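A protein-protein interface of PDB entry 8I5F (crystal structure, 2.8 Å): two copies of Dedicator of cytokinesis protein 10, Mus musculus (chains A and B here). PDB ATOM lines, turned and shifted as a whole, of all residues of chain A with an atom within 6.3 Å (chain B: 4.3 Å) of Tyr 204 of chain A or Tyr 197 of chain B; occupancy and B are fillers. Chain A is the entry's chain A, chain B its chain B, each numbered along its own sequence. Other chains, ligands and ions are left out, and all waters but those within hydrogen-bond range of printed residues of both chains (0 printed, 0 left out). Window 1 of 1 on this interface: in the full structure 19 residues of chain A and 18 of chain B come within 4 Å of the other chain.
Tyr 204 of chain A touches just these residues of chain B: Phe 190, Leu 193 and Tyr 197. Of chain A, only Tyr 197 (3.4 Å), Ile 200 (3.6 Å), His 201 (3.7 Å) and Tyr 204 (3.7 Å) come within 4 Å of Tyr 197 of chain B. Of the printed residues of chain B, Ile 200 of chain A touches Tyr 197. Of the printed residues of chain A, Phe 190 of chain B touches Tyr 204 (3.7 Å), Val 207 (3.6 Å) and Ala 208 (3.95 Å). Ile 181 of chain B touches none of the printed residues of chain A. The nearest residue of chain B that does not touch Tyr 204 of chain A is Ser 194 of chain B (4.04 Å). The nearest residue of chain A that does not touch Tyr 197 of chain B is Ala 174 of chain A (4.2 Å). The nearest printed residue of chain B that does not touch His 201 of chain A is Asp 195 of chain B (5.0 Å).
Ser 194 of chain A touches His 201 of chain B, and with the chains exchanged His 201 of chain A touches Ser 194 of chain B. Tyr 197 of chain A touches Ile 200 of chain B, and with the chains exchanged Ile 200 of chain A touches Tyr 197 of chain B. Tyr 197 of chain A touches His 201 of chain B, and with the chains exchanged His 201 of chain A touches Tyr 197 of chain B. Tyr 198 of chain A touches His 201 of chain B, and with the chains exchanged His 201 of chain A touches Tyr 198 of chain B. Of the 15 pairs that touch across the chains among the printed residues, 9 have their exchanged pair printed and touching as well.
CD1 of Tyr 197 of chain B touches CD1 of Tyr 197 of chain A (3.4 Å). Tyr 197 of chain A touches His 201 of chain B (CB to CB, 3.5 Å). Tyr 197 of chain B touches Ile 200 of chain A (CE1 to CG2, 3.6 Å). His 201 of chain A touches Tyr 197 of chain B. Tyr 198 of chain B touches His 201 of chain A. Phe 190 of chain B touches Tyr 204 of chain A (CD1 to CD1, 3.7 Å). Leu 193 of chain B touches Tyr 204 of chain A. Leu 205 of chain A touches Ser 194 of chain B. Val 207 of chain A touches Phe 190 of chain B. Ala 208 of chain A touches Phe 190 of chain B (CB to CB, 3.95 Å).
The side-chain hydroxyl (OH) of Tyr 198 of chain A sits at hydrogen-bond distance from the guanidinium group (NE) of Arg 202 of chain A, 3.2 Å away.
ND1 of His 201 of chain B is in hydrogen-bond range of O of Ser 194 of chain A, at 3.0 Å. The backbone carbonyl oxygen (O) of Ser 194 of chain B sits at hydrogen-bond distance from a ring nitrogen (ND1) of His 201 of chain A (3.1 Å).
Hydrophobic or aromatic side chains of chain A that line the printed part of chain B: Tyr 197, Tyr 198, Ile 200, His 201, Tyr 204, Leu 205, Val 207 and Ala 208. Printed residues of chain B that touch a printed residue of chain A: Phe 190, Leu 193, Ser 194, Tyr 197, Tyr 198, Ile 200 and His 201. Hydrophobic or aromatic side chains of chain B that line the printed part of chain A: Phe 190, Leu 193, Tyr 197, Tyr 198, Ile 200 and His 201. Among the printed residues, 15 pairs touch across the chains. Among the printed residues, no Asp or Glu carboxylate lies within 4 Å of a Lys or Arg side-chain nitrogen of the other chain.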
ATOM      1  N   TRP A 165     -18.781 -22.691 -12.014  1.00  0.00           N
ATOM      2  CA  TRP A 165     -20.115 -22.272 -12.393  1.00  0.00           C
ATOM      3  C   TRP A 165     -21.050 -22.515 -11.239  1.00  0.00           C
ATOM      4  O   TRP A 165     -21.612 -21.575 -10.673  1.00  0.00           O
ATOM      5  CB  TRP A 165     -20.599 -23.006 -13.655  1.00  0.00           C
ATOM      6  CG  TRP A 165     -20.420 -22.195 -14.956  1.00  0.00           C
ATOM      7  CD1 TRP A 165     -19.491 -22.406 -15.952  1.00  0.00           C
ATOM      8  CD2 TRP A 165     -21.170 -21.032 -15.369  1.00  0.00           C
ATOM      9  NE1 TRP A 165     -19.620 -21.457 -16.940  1.00  0.00           N
ATOM     10  CE2 TRP A 165     -20.644 -20.612 -16.620  1.00  0.00           C
ATOM     11  CE3 TRP A 165     -22.238 -20.313 -14.807  1.00  0.00           C
ATOM     12  CZ2 TRP A 165     -21.158 -19.513 -17.325  1.00  0.00           C
ATOM     13  CZ3 TRP A 165     -22.753 -19.214 -15.513  1.00  0.00           C
ATOM     14  CH2 TRP A 165     -22.203 -18.827 -16.764  1.00  0.00           C
ATOM     15  N   TYR A 170     -17.739 -17.099 -10.864  1.00  0.00           N
ATOM     16  CA  TYR A 170     -17.679 -16.863 -12.287  1.00  0.00           C
ATOM     17  C   TYR A 170     -16.401 -16.179 -12.760  1.00  0.00           C
ATOM     18  O   TYR A 170     -15.874 -16.529 -13.823  1.00  0.00           O
ATOM     19  CB  TYR A 170     -18.871 -16.018 -12.681  1.00  0.00           C
ATOM     20  CG  TYR A 170     -20.217 -16.519 -12.241  1.00  0.00           C
ATOM     21  CD1 TYR A 170     -20.695 -17.766 -12.634  1.00  0.00           C
ATOM     22  CD2 TYR A 170     -21.039 -15.716 -11.471  1.00  0.00           C
ATOM     23  CE1 TYR A 170     -21.966 -18.200 -12.253  1.00  0.00           C
ATOM     24  CE2 TYR A 170     -22.285 -16.128 -11.073  1.00  0.00           C
ATOM     25  CZ  TYR A 170     -22.753 -17.363 -11.460  1.00  0.00           C
ATOM     26  OH  TYR A 170     -24.014 -17.734 -11.049  1.00  0.00           O
ATOM     27  N   GLU A 171     -15.908 -15.195 -12.005  1.00  0.00           N
ATOM     28  CA  GLU A 171     -14.710 -14.445 -12.402  1.00  0.00           C
ATOM     29  C   GLU A 171     -13.478 -15.320 -12.681  1.00  0.00           C
ATOM     30  O   GLU A 171     -12.573 -14.876 -13.386  1.00  0.00           O
ATOM     31  CB  GLU A 171     -14.396 -13.383 -11.321  1.00  0.00           C
ATOM     32  CG  GLU A 171     -15.307 -12.105 -11.386  1.00  0.00           C
ATOM     33  CD  GLU A 171     -16.484 -12.013 -10.377  1.00  0.00           C
ATOM     34  OE1 GLU A 171     -17.254 -12.989 -10.202  1.00  0.00           O
ATOM     35  OE2 GLU A 171     -16.646 -10.934  -9.750  1.00  0.00           O
ATOM     36  N   ALA A 174     -12.724 -17.435 -16.972  1.00  0.00           N
ATOM     37  CA  ALA A 174     -11.790 -17.072 -18.030  1.00  0.00           C
ATOM     38  C   ALA A 174     -10.388 -17.607 -17.729  1.00  0.00           C
ATOM     39  O   ALA A 174      -9.746 -18.245 -18.591  1.00  0.00           O
ATOM     40  CB  ALA A 174     -11.754 -15.560 -18.233  1.00  0.00           C
ATOM     41  N   ASP A 175      -9.948 -17.479 -16.468  1.00  0.00           N
ATOM     42  CA  ASP A 175      -8.579 -17.870 -16.154  1.00  0.00           C
ATOM     43  C   ASP A 175      -8.380 -19.385 -16.240  1.00  0.00           C
ATOM     44  O   ASP A 175      -7.461 -19.843 -16.921  1.00  0.00           O
ATOM     45  CB  ASP A 175      -8.199 -17.360 -14.781  1.00  0.00           C
ATOM     46  CG  ASP A 175      -7.410 -16.089 -14.856  1.00  0.00           C
ATOM     47  OD1 ASP A 175      -6.813 -15.780 -15.925  1.00  0.00           O
ATOM     48  OD2 ASP A 175      -7.350 -15.409 -13.814  1.00  0.00           O
ATOM     49  N   LYS A 178      -8.216 -20.162 -19.850  1.00  0.00           N
ATOM     50  CA  LYS A 178      -7.140 -19.615 -20.681  1.00  0.00           C
ATOM     51  C   LYS A 178      -6.149 -20.656 -21.187  1.00  0.00           C
ATOM     52  O   LYS A 178      -5.840 -20.640 -22.394  1.00  0.00           O
ATOM     53  CB  LYS A 178      -6.449 -18.476 -19.931  1.00  0.00           C
ATOM     54  CG  LYS A 178      -7.118 -17.136 -20.211  1.00  0.00           C
ATOM     55  CD  LYS A 178      -6.512 -16.079 -19.338  1.00  0.00           C
ATOM     56  CE  LYS A 178      -6.968 -14.696 -19.771  1.00  0.00           C
ATOM     57  NZ  LYS A 178      -6.302 -13.610 -18.971  1.00  0.00           N
ATOM     58  N   ILE A 181      -7.765 -22.840 -24.138  1.00  0.00           N
ATOM     59  CA  ILE A 181      -7.743 -22.143 -25.406  1.00  0.00           C
ATOM     60  C   ILE A 181      -6.403 -22.336 -26.097  1.00  0.00           C
ATOM     61  O   ILE A 181      -6.342 -22.549 -27.331  1.00  0.00           O
ATOM     62  CB  ILE A 181      -8.051 -20.658 -25.177  1.00  0.00           C
ATOM     63  CG1 ILE A 181      -9.561 -20.504 -24.987  1.00  0.00           C
ATOM     64  CG2 ILE A 181      -7.500 -19.839 -26.302  1.00  0.00           C
ATOM     65  CD1 ILE A 181      -9.948 -19.332 -24.102  1.00  0.00           C
ATOM     66  N   SER A 194     -14.166 -21.653 -30.304  1.00  0.00           N
ATOM     67  CA  SER A 194     -15.323 -20.760 -30.215  1.00  0.00           C
ATOM     68  C   SER A 194     -16.194 -21.142 -29.032  1.00  0.00           C
ATOM     69  O   SER A 194     -16.730 -20.264 -28.340  1.00  0.00           O
ATOM     70  CB  SER A 194     -16.118 -20.676 -31.520  1.00  0.00           C
ATOM     71  OG  SER A 194     -16.937 -21.787 -31.656  1.00  0.00           O
ATOM     72  N   LEU A 196     -15.094 -22.501 -26.114  1.00  0.00           N
ATOM     73  CA  LEU A 196     -14.368 -21.910 -24.986  1.00  0.00           C
ATOM     74  C   LEU A 196     -14.597 -20.402 -24.838  1.00  0.00           C
ATOM     75  O   LEU A 196     -14.794 -19.892 -23.717  1.00  0.00           O
ATOM     76  CB  LEU A 196     -12.869 -22.179 -25.163  1.00  0.00           C
ATOM     77  CG  LEU A 196     -12.476 -23.659 -25.102  1.00  0.00           C
ATOM     78  CD1 LEU A 196     -11.068 -23.872 -25.597  1.00  0.00           C
ATOM     79  CD2 LEU A 196     -12.653 -24.174 -23.664  1.00  0.00           C
ATOM     80  N   TYR A 197     -14.596 -19.668 -25.961  1.00  0.00           N
ATOM     81  CA  TYR A 197     -14.764 -18.218 -25.890  1.00  0.00           C
ATOM     82  C   TYR A 197     -16.199 -17.855 -25.560  1.00  0.00           C
ATOM     83  O   TYR A 197     -16.457 -16.970 -24.742  1.00  0.00           O
ATOM     84  CB  TYR A 197     -14.343 -17.569 -27.221  1.00  0.00           C
ATOM     85  CG  TYR A 197     -12.906 -17.244 -27.175  1.00  0.00           C
ATOM     86  CD1 TYR A 197     -12.469 -16.041 -26.644  1.00  0.00           C
ATOM     87  CD2 TYR A 197     -11.978 -18.187 -27.532  1.00  0.00           C
ATOM     88  CE1 TYR A 197     -11.119 -15.771 -26.512  1.00  0.00           C
ATOM     89  CE2 TYR A 197     -10.663 -17.945 -27.406  1.00  0.00           C
ATOM     90  CZ  TYR A 197     -10.225 -16.746 -26.893  1.00  0.00           C
ATOM     91  OH  TYR A 197      -8.877 -16.565 -26.792  1.00  0.00           O
ATOM     92  N   TYR A 198     -17.141 -18.575 -26.130  1.00  0.00           N
ATOM     93  CA  TYR A 198     -18.531 -18.338 -25.805  1.00  0.00           C
ATOM     94  C   TYR A 198     -18.781 -18.605 -24.315  1.00  0.00           C
ATOM     95  O   TYR A 198     -19.499 -17.852 -23.649  1.00  0.00           O
ATOM     96  CB  TYR A 198     -19.378 -19.222 -26.711  1.00  0.00           C
ATOM     97  CG  TYR A 198     -20.839 -19.144 -26.501  1.00  0.00           C
ATOM     98  CD1 TYR A 198     -21.556 -18.044 -26.902  1.00  0.00           C
ATOM     99  CD2 TYR A 198     -21.509 -20.167 -25.802  1.00  0.00           C
ATOM    100  CE1 TYR A 198     -22.951 -17.978 -26.714  1.00  0.00           C
ATOM    101  CE2 TYR A 198     -22.880 -20.117 -25.581  1.00  0.00           C
ATOM    102  CZ  TYR A 198     -23.600 -19.013 -26.051  1.00  0.00           C
ATOM    103  OH  TYR A 198     -24.961 -18.952 -25.828  1.00  0.00           O
ATOM    104  N   ASP A 199     -18.246 -19.710 -23.794  1.00  0.00           N
ATOM    105  CA  ASP A 199     -18.363 -20.009 -22.375  1.00  0.00           C
ATOM    106  C   ASP A 199     -17.860 -18.827 -21.553  1.00  0.00           C
ATOM    107  O   ASP A 199     -18.599 -18.270 -20.738  1.00  0.00           O
ATOM    108  CB  ASP A 199     -17.594 -21.305 -22.046  1.00  0.00           C
ATOM    109  CG  ASP A 199     -17.676 -21.700 -20.544  1.00  0.00           C
ATOM    110  OD1 ASP A 199     -18.823 -21.837 -20.044  1.00  0.00           O
ATOM    111  OD2 ASP A 199     -16.598 -21.862 -19.881  1.00  0.00           O
ATOM    112  N   ILE A 200     -16.620 -18.402 -21.787  1.00  0.00           N
ATOM    113  CA  ILE A 200     -16.119 -17.275 -21.009  1.00  0.00           C
ATOM    114  C   ILE A 200     -17.050 -16.077 -21.140  1.00  0.00           C
ATOM    115  O   ILE A 200     -17.248 -15.304 -20.188  1.00  0.00           O
ATOM    116  CB  ILE A 200     -14.695 -16.915 -21.441  1.00  0.00           C
ATOM    117  CG1 ILE A 200     -13.825 -18.172 -21.435  1.00  0.00           C
ATOM    118  CG2 ILE A 200     -14.152 -15.809 -20.574  1.00  0.00           C
ATOM    119  CD1 ILE A 200     -12.356 -17.843 -21.527  1.00  0.00           C
ATOM    120  N   HIS A 201     -17.612 -15.893 -22.332  1.00  0.00           N
ATOM    121  CA  HIS A 201     -18.527 -14.789 -22.572  1.00  0.00           C
ATOM    122  C   HIS A 201     -19.737 -14.877 -21.654  1.00  0.00           C
ATOM    123  O   HIS A 201     -19.990 -13.952 -20.881  1.00  0.00           O
ATOM    124  CB  HIS A 201     -18.926 -14.782 -24.048  1.00  0.00           C
ATOM    125  CG  HIS A 201     -20.346 -14.391 -24.311  1.00  0.00           C
ATOM    126  ND1 HIS A 201     -20.803 -13.096 -24.184  1.00  0.00           N
ATOM    127  CD2 HIS A 201     -21.411 -15.130 -24.707  1.00  0.00           C
ATOM    128  CE1 HIS A 201     -22.092 -13.059 -24.474  1.00  0.00           C
ATOM    129  NE2 HIS A 201     -22.485 -14.280 -24.794  1.00  0.00           N
ATOM    130  N   ARG A 202     -20.471 -15.999 -21.708  1.00  0.00           N
ATOM    131  CA  ARG A 202     -21.589 -16.254 -20.787  1.00  0.00           C
ATOM    132  C   ARG A 202     -21.167 -16.050 -19.333  1.00  0.00           C
ATOM    133  O   ARG A 202     -21.968 -15.612 -18.496  1.00  0.00           O
ATOM    134  CB  ARG A 202     -22.118 -17.694 -20.953  1.00  0.00           C
ATOM    135  CG  ARG A 202     -22.437 -18.133 -22.358  1.00  0.00           C
ATOM    136  CD  ARG A 202     -23.402 -17.264 -22.950  1.00  0.00           C
ATOM    137  NE  ARG A 202     -24.765 -17.756 -22.882  1.00  0.00           N
ATOM    138  CZ  ARG A 202     -25.675 -17.338 -22.020  1.00  0.00           C
ATOM    139  NH1 ARG A 202     -25.336 -16.464 -21.087  1.00  0.00           N
ATOM    140  NH2 ARG A 202     -26.908 -17.808 -22.079  1.00  0.00           N
ATOM    141  N   SER A 203     -19.901 -16.311 -19.030  1.00  0.00           N
ATOM    142  CA  SER A 203     -19.428 -16.197 -17.657  1.00  0.00           C
ATOM    143  C   SER A 203     -19.392 -14.729 -17.222  1.00  0.00           C
ATOM    144  O   SER A 203     -19.937 -14.361 -16.177  1.00  0.00           O
ATOM    145  CB  SER A 203     -18.062 -16.892 -17.533  1.00  0.00           C
ATOM    146  OG  SER A 203     -17.250 -16.344 -16.493  1.00  0.00           O
ATOM    147  N   TYR A 204     -18.804 -13.861 -18.038  1.00  0.00           N
ATOM    148  CA  TYR A 204     -18.855 -12.439 -17.687  1.00  0.00           C
ATOM    149  C   TYR A 204     -20.230 -11.857 -17.875  1.00  0.00           C
ATOM    150  O   TYR A 204     -20.552 -10.873 -17.229  1.00  0.00           O
ATOM    151  CB  TYR A 204     -17.913 -11.596 -18.512  1.00  0.00           C
ATOM    152  CG  TYR A 204     -16.485 -11.815 -18.173  1.00  0.00           C
ATOM    153  CD1 TYR A 204     -15.959 -11.358 -16.969  1.00  0.00           C
ATOM    154  CD2 TYR A 204     -15.652 -12.481 -19.044  1.00  0.00           C
ATOM    155  CE1 TYR A 204     -14.644 -11.558 -16.649  1.00  0.00           C
ATOM    156  CE2 TYR A 204     -14.335 -12.674 -18.742  1.00  0.00           C
ATOM    157  CZ  TYR A 204     -13.832 -12.222 -17.545  1.00  0.00           C
ATOM    158  OH  TYR A 204     -12.496 -12.443 -17.278  1.00  0.00           O
ATOM    159  N   LEU A 205     -21.048 -12.436 -18.733  1.00  0.00           N
ATOM    160  CA  LEU A 205     -22.421 -11.984 -18.827  1.00  0.00           C
ATOM    161  C   LEU A 205     -23.090 -12.105 -17.480  1.00  0.00           C
ATOM    162  O   LEU A 205     -23.639 -11.129 -16.945  1.00  0.00           O
ATOM    163  CB  LEU A 205     -23.140 -12.804 -19.877  1.00  0.00           C
ATOM    164  CG  LEU A 205     -24.430 -12.289 -20.454  1.00  0.00           C
ATOM    165  CD1 LEU A 205     -24.194 -10.854 -20.778  1.00  0.00           C
ATOM    166  CD2 LEU A 205     -24.697 -13.083 -21.725  1.00  0.00           C
ATOM    167  N   LYS A 206     -22.984 -13.299 -16.880  1.00  0.00           N
ATOM    168  CA  LYS A 206     -23.481 -13.519 -15.523  1.00  0.00           C
ATOM    169  C   LYS A 206     -22.869 -12.502 -14.555  1.00  0.00           C
ATOM    170  O   LYS A 206     -23.583 -11.847 -13.773  1.00  0.00           O
ATOM    171  CB  LYS A 206     -23.172 -14.948 -15.093  1.00  0.00           C
ATOM    172  CG  LYS A 206     -23.993 -15.410 -13.913  1.00  0.00           C
ATOM    173  CD  LYS A 206     -25.452 -15.497 -14.347  1.00  0.00           C
ATOM    174  CE  LYS A 206     -26.391 -15.817 -13.206  1.00  0.00           C
ATOM    175  NZ  LYS A 206     -27.808 -15.848 -13.689  1.00  0.00           N
ATOM    176  N   VAL A 207     -21.537 -12.394 -14.557  1.00  0.00           N
ATOM    177  CA  VAL A 207     -20.915 -11.504 -13.586  1.00  0.00           C
ATOM    178  C   VAL A 207     -21.516 -10.113 -13.695  1.00  0.00           C
ATOM    179  O   VAL A 207     -21.868  -9.492 -12.687  1.00  0.00           O
ATOM    180  CB  VAL A 207     -19.392 -11.470 -13.757  1.00  0.00           C
ATOM    181  CG1 VAL A 207     -18.824 -10.510 -12.752  1.00  0.00           C
ATOM    182  CG2 VAL A 207     -18.839 -12.831 -13.480  1.00  0.00           C
ATOM    183  N   ALA A 208     -21.681  -9.621 -14.930  1.00  0.00           N
ATOM    184  CA  ALA A 208     -22.250  -8.296 -15.148  1.00  0.00           C
ATOM    185  C   ALA A 208     -23.650  -8.201 -14.568  1.00  0.00           C
ATOM    186  O   ALA A 208     -24.016  -7.196 -13.942  1.00  0.00           O
ATOM    187  CB  ALA A 208     -22.269  -8.005 -16.638  1.00  0.00           C
ATOM    188  N   GLU A 209     -24.436  -9.258 -14.764  1.00  0.00           N
ATOM    189  CA  GLU A 209     -25.776  -9.342 -14.192  1.00  0.00           C
ATOM    190  C   GLU A 209     -25.770  -9.174 -12.665  1.00  0.00           C
ATOM    191  O   GLU A 209     -26.599  -8.436 -12.116  1.00  0.00           O
ATOM    192  CB  GLU A 209     -26.414 -10.670 -14.590  1.00  0.00           C
ATOM    193  CG  GLU A 209     -27.642 -11.032 -13.775  1.00  0.00           C
ATOM    194  CD  GLU A 209     -28.218 -12.389 -14.168  1.00  0.00           C
ATOM    195  OE1 GLU A 209     -28.967 -12.995 -13.345  1.00  0.00           O
ATOM    196  OE2 GLU A 209     -27.948 -12.825 -15.318  1.00  0.00           O
ATOM    197  N   ILE B 181      -8.821  -6.823 -23.904  1.00  0.00           N
ATOM    198  CA  ILE B 181      -9.364  -7.534 -22.742  1.00  0.00           C
ATOM    199  C   ILE B 181      -8.590  -7.176 -21.472  1.00  0.00           C
ATOM    200  O   ILE B 181      -9.190  -6.941 -20.409  1.00  0.00           O
ATOM    201  CB  ILE B 181      -9.396  -9.062 -22.965  1.00  0.00           C
ATOM    202  CG1 ILE B 181     -10.601  -9.505 -23.835  1.00  0.00           C
ATOM    203  CG2 ILE B 181      -9.336  -9.813 -21.631  1.00  0.00           C
ATOM    204  CD1 ILE B 181     -10.379 -10.778 -24.635  1.00  0.00           C
ATOM    205  N   PHE B 190     -17.212  -5.600 -16.837  1.00  0.00           N
ATOM    206  CA  PHE B 190     -17.618  -6.930 -17.260  1.00  0.00           C
ATOM    207  C   PHE B 190     -18.446  -6.903 -18.529  1.00  0.00           C
ATOM    208  O   PHE B 190     -18.274  -7.786 -19.367  1.00  0.00           O
ATOM    209  CB  PHE B 190     -18.363  -7.657 -16.132  1.00  0.00           C
ATOM    210  CG  PHE B 190     -17.579  -7.701 -14.849  1.00  0.00           C
ATOM    211  CD1 PHE B 190     -16.360  -8.340 -14.800  1.00  0.00           C
ATOM    212  CD2 PHE B 190     -18.054  -7.102 -13.703  1.00  0.00           C
ATOM    213  CE1 PHE B 190     -15.643  -8.367 -13.647  1.00  0.00           C
ATOM    214  CE2 PHE B 190     -17.331  -7.151 -12.530  1.00  0.00           C
ATOM    215  CZ  PHE B 190     -16.135  -7.783 -12.500  1.00  0.00           C
ATOM    216  N   LEU B 193     -15.820  -6.928 -21.290  1.00  0.00           N
ATOM    217  CA  LEU B 193     -15.306  -8.299 -21.342  1.00  0.00           C
ATOM    218  C   LEU B 193     -16.288  -9.236 -22.045  1.00  0.00           C
ATOM    219  O   LEU B 193     -15.893 -10.078 -22.863  1.00  0.00           O
ATOM    220  CB  LEU B 193     -14.926  -8.798 -19.950  1.00  0.00           C
ATOM    221  CG  LEU B 193     -13.605  -8.151 -19.475  1.00  0.00           C
ATOM    222  CD1 LEU B 193     -13.329  -8.571 -18.049  1.00  0.00           C
ATOM    223  CD2 LEU B 193     -12.398  -8.520 -20.307  1.00  0.00           C
ATOM    224  N   SER B 194     -17.568  -9.136 -21.703  1.00  0.00           N
ATOM    225  CA  SER B 194     -18.509 -10.065 -22.283  1.00  0.00           C
ATOM    226  C   SER B 194     -18.634  -9.842 -23.788  1.00  0.00           C
ATOM    227  O   SER B 194     -18.699 -10.809 -24.572  1.00  0.00           O
ATOM    228  CB  SER B 194     -19.858  -9.859 -21.620  1.00  0.00           C
ATOM    229  OG  SER B 194     -20.858 -10.498 -22.379  1.00  0.00           O
ATOM    230  N   ASP B 195     -18.646  -8.568 -24.202  1.00  0.00           N
ATOM    231  CA  ASP B 195     -18.656  -8.249 -25.617  1.00  0.00           C
ATOM    232  C   ASP B 195     -17.419  -8.792 -26.310  1.00  0.00           C
ATOM    233  O   ASP B 195     -17.500  -9.444 -27.356  1.00  0.00           O
ATOM    234  CB  ASP B 195     -18.761  -6.732 -25.829  1.00  0.00           C
ATOM    235  CG  ASP B 195     -20.057  -6.148 -25.298  1.00  0.00           C
ATOM    236  OD1 ASP B 195     -21.065  -6.863 -25.367  1.00  0.00           O
ATOM    237  OD2 ASP B 195     -20.107  -4.956 -24.885  1.00  0.00           O
ATOM    238  N   LEU B 196     -16.259  -8.443 -25.787  1.00  0.00           N
ATOM    239  CA  LEU B 196     -15.000  -8.960 -26.319  1.00  0.00           C
ATOM    240  C   LEU B 196     -14.953 -10.476 -26.451  1.00  0.00           C
ATOM    241  O   LEU B 196     -14.550 -11.001 -27.491  1.00  0.00           O
ATOM    242  CB  LEU B 196     -13.841  -8.466 -25.440  1.00  0.00           C
ATOM    243  CG  LEU B 196     -13.696  -6.933 -25.534  1.00  0.00           C
ATOM    244  CD1 LEU B 196     -12.829  -6.419 -24.384  1.00  0.00           C
ATOM    245  CD2 LEU B 196     -13.291  -6.330 -26.888  1.00  0.00           C
ATOM    246  N   TYR B 197     -15.442 -11.203 -25.464  1.00  0.00           N
ATOM    247  CA  TYR B 197     -15.325 -12.656 -25.571  1.00  0.00           C
ATOM    248  C   TYR B 197     -16.298 -13.192 -26.594  1.00  0.00           C
ATOM    249  O   TYR B 197     -15.975 -14.112 -27.357  1.00  0.00           O
ATOM    250  CB  TYR B 197     -15.512 -13.335 -24.222  1.00  0.00           C
ATOM    251  CG  TYR B 197     -14.169 -13.403 -23.540  1.00  0.00           C
ATOM    252  CD1 TYR B 197     -13.264 -14.437 -23.766  1.00  0.00           C
ATOM    253  CD2 TYR B 197     -13.808 -12.405 -22.656  1.00  0.00           C
ATOM    254  CE1 TYR B 197     -12.028 -14.445 -23.121  1.00  0.00           C
ATOM    255  CE2 TYR B 197     -12.627 -12.420 -22.017  1.00  0.00           C
ATOM    256  CZ  TYR B 197     -11.730 -13.410 -22.247  1.00  0.00           C
ATOM    257  OH  TYR B 197     -10.539 -13.320 -21.560  1.00  0.00           O
ATOM    258  N   TYR B 198     -17.488 -12.607 -26.632  1.00  0.00           N
ATOM    259  CA  TYR B 198     -18.459 -12.997 -27.634  1.00  0.00           C
ATOM    260  C   TYR B 198     -17.903 -12.735 -29.026  1.00  0.00           C
ATOM    261  O   TYR B 198     -18.086 -13.550 -29.937  1.00  0.00           O
ATOM    262  CB  TYR B 198     -19.728 -12.195 -27.410  1.00  0.00           C
ATOM    263  CG  TYR B 198     -20.818 -12.468 -28.384  1.00  0.00           C
ATOM    264  CD1 TYR B 198     -21.516 -13.659 -28.326  1.00  0.00           C
ATOM    265  CD2 TYR B 198     -21.175 -11.538 -29.368  1.00  0.00           C
ATOM    266  CE1 TYR B 198     -22.547 -13.925 -29.198  1.00  0.00           C
ATOM    267  CE2 TYR B 198     -22.215 -11.806 -30.254  1.00  0.00           C
ATOM    268  CZ  TYR B 198     -22.873 -13.012 -30.164  1.00  0.00           C
ATOM    269  OH  TYR B 198     -23.889 -13.333 -31.012  1.00  0.00           O
ATOM    270  N   ASP B 199     -17.292 -11.569 -29.226  1.00  0.00           N
ATOM    271  CA  ASP B 199     -16.671 -11.261 -30.503  1.00  0.00           C
ATOM    272  C   ASP B 199     -15.647 -12.335 -30.904  1.00  0.00           C
ATOM    273  O   ASP B 199     -15.758 -12.934 -31.980  1.00  0.00           O
ATOM    274  CB  ASP B 199     -16.063  -9.857 -30.443  1.00  0.00           C
ATOM    275  CG  ASP B 199     -17.136  -8.750 -30.136  1.00  0.00           C
ATOM    276  OD1 ASP B 199     -18.360  -8.983 -30.356  1.00  0.00           O
ATOM    277  OD2 ASP B 199     -16.745  -7.617 -29.704  1.00  0.00           O
ATOM    278  N   ILE B 200     -14.641 -12.600 -30.065  1.00  0.00           N
ATOM    279  CA  ILE B 200     -13.665 -13.638 -30.432  1.00  0.00           C
ATOM    280  C   ILE B 200     -14.360 -14.978 -30.708  1.00  0.00           C
ATOM    281  O   ILE B 200     -13.915 -15.799 -31.531  1.00  0.00           O
ATOM    282  CB  ILE B 200     -12.581 -13.794 -29.362  1.00  0.00           C
ATOM    283  CG1 ILE B 200     -11.953 -12.444 -28.975  1.00  0.00           C
ATOM    284  CG2 ILE B 200     -11.590 -14.867 -29.790  1.00  0.00           C
ATOM    285  CD1 ILE B 200     -10.621 -12.617 -28.204  1.00  0.00           C
ATOM    286  N   HIS B 201     -15.404 -15.268 -29.944  1.00  0.00           N
ATOM    287  CA  HIS B 201     -16.130 -16.502 -30.167  1.00  0.00           C
ATOM    288  C   HIS B 201     -16.717 -16.551 -31.568  1.00  0.00           C
ATOM    289  O   HIS B 201     -16.471 -17.490 -32.323  1.00  0.00           O
ATOM    290  CB  HIS B 201     -17.201 -16.680 -29.074  1.00  0.00           C
ATOM    291  CG  HIS B 201     -18.471 -17.245 -29.598  1.00  0.00           C
ATOM    292  ND1 HIS B 201     -18.594 -18.554 -30.009  1.00  0.00           N
ATOM    293  CD2 HIS B 201     -19.698 -16.685 -29.752  1.00  0.00           C
ATOM    294  CE1 HIS B 201     -19.828 -18.765 -30.441  1.00  0.00           C
ATOM    295  NE2 HIS B 201     -20.526 -17.654 -30.274  1.00  0.00           N
